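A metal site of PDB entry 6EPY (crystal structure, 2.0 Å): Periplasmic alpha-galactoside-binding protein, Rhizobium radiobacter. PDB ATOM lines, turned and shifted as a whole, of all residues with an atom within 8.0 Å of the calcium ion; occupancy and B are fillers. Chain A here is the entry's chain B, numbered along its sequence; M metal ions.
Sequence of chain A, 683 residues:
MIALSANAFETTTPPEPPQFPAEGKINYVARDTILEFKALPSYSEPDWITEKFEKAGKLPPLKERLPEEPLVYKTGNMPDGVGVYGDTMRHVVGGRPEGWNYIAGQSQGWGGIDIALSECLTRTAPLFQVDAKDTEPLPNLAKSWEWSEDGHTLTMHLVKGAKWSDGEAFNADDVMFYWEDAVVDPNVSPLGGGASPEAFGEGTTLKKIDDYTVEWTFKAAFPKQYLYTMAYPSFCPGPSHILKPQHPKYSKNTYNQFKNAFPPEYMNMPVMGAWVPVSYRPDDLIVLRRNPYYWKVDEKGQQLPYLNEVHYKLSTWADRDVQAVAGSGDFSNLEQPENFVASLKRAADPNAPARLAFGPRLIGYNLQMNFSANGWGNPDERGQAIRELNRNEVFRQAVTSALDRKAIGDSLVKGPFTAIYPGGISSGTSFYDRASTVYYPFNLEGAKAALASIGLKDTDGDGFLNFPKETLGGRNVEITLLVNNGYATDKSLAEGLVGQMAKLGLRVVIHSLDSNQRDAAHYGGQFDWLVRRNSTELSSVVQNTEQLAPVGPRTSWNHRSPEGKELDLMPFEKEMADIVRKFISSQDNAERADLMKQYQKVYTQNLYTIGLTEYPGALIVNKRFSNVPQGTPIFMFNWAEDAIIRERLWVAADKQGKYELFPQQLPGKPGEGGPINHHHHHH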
ATOM      1  N   LYS A 457     -24.625  17.033   0.227  1.00  0.00           N
ATOM      2  CA  LYS A 457     -26.069  17.209   0.390  1.00  0.00           C
ATOM      3  C   LYS A 457     -26.454  17.598   1.815  1.00  0.00           C
ATOM      4  O   LYS A 457     -25.755  17.237   2.775  1.00  0.00           O
ATOM      5  CB  LYS A 457     -26.872  15.989  -0.108  1.00  0.00           C
ATOM      6  CG  LYS A 457     -26.850  14.725   0.751  1.00  0.00           C
ATOM      7  CD  LYS A 457     -27.680  13.579   0.128  1.00  0.00           C
ATOM      8  CE  LYS A 457     -29.173  13.510   0.461  1.00  0.00           C
ATOM      9  NZ  LYS A 457     -29.498  12.466   1.457  1.00  0.00           N
ATOM     10  N   ASP A 458     -27.541  18.345   1.953  1.00  0.00           N
ATOM     11  CA  ASP A 458     -28.036  18.781   3.251  1.00  0.00           C
ATOM     12  C   ASP A 458     -28.731  17.587   3.919  1.00  0.00           C
ATOM     13  O   ASP A 458     -29.743  17.103   3.413  1.00  0.00           O
ATOM     14  CB  ASP A 458     -28.983  19.977   3.096  1.00  0.00           C
ATOM     15  CG  ASP A 458     -29.552  20.548   4.378  1.00  0.00           C
ATOM     16  OD1 ASP A 458     -28.935  20.354   5.444  1.00  0.00           O
ATOM     17  OD2 ASP A 458     -30.592  21.226   4.299  1.00  0.00           O
ATOM     18  N   THR A 459     -28.126  17.077   5.010  1.00  0.00           N
ATOM     19  CA  THR A 459     -28.618  15.900   5.749  1.00  0.00           C
ATOM     20  C   THR A 459     -29.268  16.258   7.095  1.00  0.00           C
ATOM     21  O   THR A 459     -29.695  15.360   7.814  1.00  0.00           O
ATOM     22  CB  THR A 459     -27.500  14.854   5.888  1.00  0.00           C
ATOM     23  OG1 THR A 459     -26.385  15.432   6.573  1.00  0.00           O
ATOM     24  CG2 THR A 459     -27.033  14.284   4.546  1.00  0.00           C
ATOM     25  N   ASP A 460     -29.355  17.566   7.434  1.00  0.00           N
ATOM     26  CA  ASP A 460     -29.946  18.003   8.708  1.00  0.00           C
ATOM     27  C   ASP A 460     -31.028  19.118   8.533  1.00  0.00           C
ATOM     28  O   ASP A 460     -31.463  19.730   9.517  1.00  0.00           O
ATOM     29  CB  ASP A 460     -28.845  18.417   9.720  1.00  0.00           C
ATOM     30  CG  ASP A 460     -27.752  19.326   9.198  1.00  0.00           C
ATOM     31  OD1 ASP A 460     -28.073  20.261   8.427  1.00  0.00           O
ATOM     32  OD2 ASP A 460     -26.582  19.148   9.589  1.00  0.00           O
ATOM     33  N   GLY A 461     -31.458  19.323   7.283  1.00  0.00           N
ATOM     34  CA  GLY A 461     -32.482  20.298   6.900  1.00  0.00           C
ATOM     35  C   GLY A 461     -32.236  21.775   7.179  1.00  0.00           C
ATOM     36  O   GLY A 461     -33.186  22.557   7.162  1.00  0.00           O
ATOM     37  N   ASP A 462     -30.980  22.192   7.408  1.00  0.00           N
ATOM     38  CA  ASP A 462     -30.716  23.604   7.687  1.00  0.00           C
ATOM     39  C   ASP A 462     -30.401  24.448   6.417  1.00  0.00           C
ATOM     40  O   ASP A 462     -30.031  25.610   6.531  1.00  0.00           O
ATOM     41  CB  ASP A 462     -29.614  23.777   8.767  1.00  0.00           C
ATOM     42  CG  ASP A 462     -28.183  23.429   8.388  1.00  0.00           C
ATOM     43  OD1 ASP A 462     -27.969  22.883   7.276  1.00  0.00           O
ATOM     44  OD2 ASP A 462     -27.287  23.653   9.218  1.00  0.00           O
ATOM     45  N   GLY A 463     -30.550  23.852   5.238  1.00  0.00           N
ATOM     46  CA  GLY A 463     -30.293  24.546   3.971  1.00  0.00           C
ATOM     47  C   GLY A 463     -28.838  24.583   3.534  1.00  0.00           C
ATOM     48  O   GLY A 463     -28.533  25.018   2.421  1.00  0.00           O
ATOM     49  N   PHE A 464     -27.916  24.119   4.402  1.00  0.00           N
ATOM     50  CA  PHE A 464     -26.489  24.067   4.117  1.00  0.00           C
ATOM     51  C   PHE A 464     -26.018  22.645   3.868  1.00  0.00           C
ATOM     52  O   PHE A 464     -26.418  21.722   4.581  1.00  0.00           O
ATOM     53  CB  PHE A 464     -25.676  24.737   5.227  1.00  0.00           C
ATOM     54  CG  PHE A 464     -25.858  26.240   5.245  1.00  0.00           C
ATOM     55  CD1 PHE A 464     -25.255  27.039   4.287  1.00  0.00           C
ATOM     56  CD2 PHE A 464     -26.655  26.848   6.208  1.00  0.00           C
ATOM     57  CE1 PHE A 464     -25.405  28.426   4.301  1.00  0.00           C
ATOM     58  CE2 PHE A 464     -26.821  28.242   6.214  1.00  0.00           C
ATOM     59  CZ  PHE A 464     -26.177  29.022   5.275  1.00  0.00           C
ATOM     60  N   LEU A 465     -25.179  22.480   2.840  1.00  0.00           N
ATOM     61  CA  LEU A 465     -24.673  21.178   2.456  1.00  0.00           C
ATOM     62  C   LEU A 465     -23.704  20.599   3.467  1.00  0.00           C
ATOM     63  O   LEU A 465     -22.856  21.321   4.021  1.00  0.00           O
ATOM     64  CB  LEU A 465     -24.039  21.225   1.053  1.00  0.00           C
ATOM     65  CG  LEU A 465     -24.933  21.739  -0.079  1.00  0.00           C
ATOM     66  CD1 LEU A 465     -24.118  22.156  -1.252  1.00  0.00           C
ATOM     67  CD2 LEU A 465     -25.960  20.701  -0.483  1.00  0.00           C
ATOM     68  N   ASN A 466     -23.871  19.304   3.731  1.00  0.00           N
ATOM     69  CA  ASN A 466     -23.059  18.517   4.646  1.00  0.00           C
ATOM     70  C   ASN A 466     -22.071  17.682   3.871  1.00  0.00           C
ATOM     71  O   ASN A 466     -22.362  17.258   2.731  1.00  0.00           O
ATOM     72  CB  ASN A 466     -23.952  17.560   5.459  1.00  0.00           C
ATOM     73  CG  ASN A 466     -24.853  18.252   6.418  1.00  0.00           C
ATOM     74  OD1 ASN A 466     -25.847  18.880   6.041  1.00  0.00           O
ATOM     75  ND2 ASN A 466     -24.561  18.117   7.700  1.00  0.00           N
ATOM     76  N   PHE A 467     -20.929  17.375   4.500  1.00  0.00           N
ATOM     77  CA  PHE A 467     -19.964  16.453   3.944  1.00  0.00           C
ATOM     78  C   PHE A 467     -20.600  15.052   4.007  1.00  0.00           C
ATOM     79  O   PHE A 467     -21.469  14.832   4.875  1.00  0.00           O
ATOM     80  CB  PHE A 467     -18.704  16.404   4.828  1.00  0.00           C
ATOM     81  CG  PHE A 467     -17.754  17.558   4.644  1.00  0.00           C
ATOM     82  CD1 PHE A 467     -16.930  17.629   3.522  1.00  0.00           C
ATOM     83  CD2 PHE A 467     -17.624  18.530   5.619  1.00  0.00           C
ATOM     84  CE1 PHE A 467     -16.029  18.686   3.374  1.00  0.00           C
ATOM     85  CE2 PHE A 467     -16.716  19.594   5.462  1.00  0.00           C
ATOM     86  CZ  PHE A 467     -15.912  19.653   4.346  1.00  0.00           C
ATOM     87  N   GLY A 474     -19.856  13.887   8.864  1.00  0.00           N
ATOM     88  CA  GLY A 474     -21.008  14.346   8.098  1.00  0.00           C
ATOM     89  C   GLY A 474     -21.518  15.726   8.440  1.00  0.00           C
ATOM     90  O   GLY A 474     -22.669  16.055   8.129  1.00  0.00           O
ATOM     91  N   ARG A 475     -20.680  16.569   9.082  1.00  0.00           N
ATOM     92  CA  ARG A 475     -21.053  17.929   9.468  1.00  0.00           C
ATOM     93  C   ARG A 475     -21.190  18.861   8.253  1.00  0.00           C
ATOM     94  O   ARG A 475     -20.755  18.499   7.156  1.00  0.00           O
ATOM     95  CB  ARG A 475     -20.036  18.528  10.483  1.00  0.00           C
ATOM     96  CG  ARG A 475     -18.737  18.975   9.838  1.00  0.00           C
ATOM     97  CD  ARG A 475     -17.790  19.542  10.868  1.00  0.00           C
ATOM     98  NE  ARG A 475     -17.155  18.465  11.623  1.00  0.00           N
ATOM     99  CZ  ARG A 475     -15.975  18.538  12.210  1.00  0.00           C
ATOM    100  NH1 ARG A 475     -15.276  19.677  12.166  1.00  0.00           N
ATOM    101  NH2 ARG A 475     -15.467  17.493  12.835  1.00  0.00           N
ATOM    102  N   ASN A 476     -21.761  20.052   8.464  1.00  0.00           N
ATOM    103  CA  ASN A 476     -21.878  21.062   7.434  1.00  0.00           C
ATOM    104  C   ASN A 476     -20.515  21.484   6.906  1.00  0.00           C
ATOM    105  O   ASN A 476     -19.555  21.609   7.684  1.00  0.00           O
ATOM    106  CB  ASN A 476     -22.593  22.306   7.951  1.00  0.00           C
ATOM    107  CG  ASN A 476     -24.097  22.225   7.967  1.00  0.00           C
ATOM    108  OD1 ASN A 476     -24.715  21.480   7.208  1.00  0.00           O
ATOM    109  ND2 ASN A 476     -24.696  23.052   8.798  1.00  0.00           N
ATOM    110  N   VAL A 477     -20.430  21.691   5.581  1.00  0.00           N
ATOM    111  CA  VAL A 477     -19.251  22.229   4.948  1.00  0.00           C
ATOM    112  C   VAL A 477     -19.164  23.696   5.454  1.00  0.00           C
ATOM    113  O   VAL A 477     -20.167  24.425   5.421  1.00  0.00           O
ATOM    114  CB  VAL A 477     -19.356  22.181   3.396  1.00  0.00           C
ATOM    115  CG1 VAL A 477     -18.142  22.856   2.721  1.00  0.00           C
ATOM    116  CG2 VAL A 477     -19.527  20.744   2.895  1.00  0.00           C
ATOM    117  N   GLY A 505     -25.933  26.632  -1.225  1.00  0.00           N
ATOM    118  CA  GLY A 505     -25.940  25.756  -0.054  1.00  0.00           C
ATOM    119  C   GLY A 505     -24.605  25.639   0.656  1.00  0.00           C
ATOM    120  O   GLY A 505     -24.461  24.796   1.537  1.00  0.00           O
HETATM  121 CA    CA M   1     -26.968  20.980   6.602  1.00  0.00          CA
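OD2 of Asp 458 sits at hydrogen-bond distance from N of Gly 463, at 2.8 Å.
OD1 of Asp 458 sits close to N of Gly 461 (3.3 Å).
The side-chain amide nitrogen of Asn 466 sits close to the side-chain hydroxyl of Thr 459 (3.4 Å).
The backbone NH of Asn 466 sits at hydrogen-bond distance from the backbone carbonyl oxygen of Lys 457 (3.0 Å).
The side-chain amide nitrogen of Asn 466 lies within hydrogen-bond range of the backbone carbonyl oxygen of Gly 474 (2.8 Å).
Of the 16 residues printed, 6 come within 4 Å of the calcium ion.
Along chain A the residues within 4 Å of the calcium ion span positions 458 to 476.
The calcium ion is bound by the backbone carbonyl oxygen (O) of Phe 464, 2.2 Å away.
OD1 of Asp 460 is bound to the calcium ion (2.3 Å).
The calcium ion is bound by the side-chain carboxylate (OD1) of Asp 462 (2.3 Å).
OD1 of Asp 458 binds the calcium ion, 2.4 Å away.
The side-chain amide oxygen (OD1) of Asn 476 binds the calcium ion.
The calcium ion is bound by OD1 of Asn 466, at 2.4 Å.
The calcium ion has six donor atoms within binding distance.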
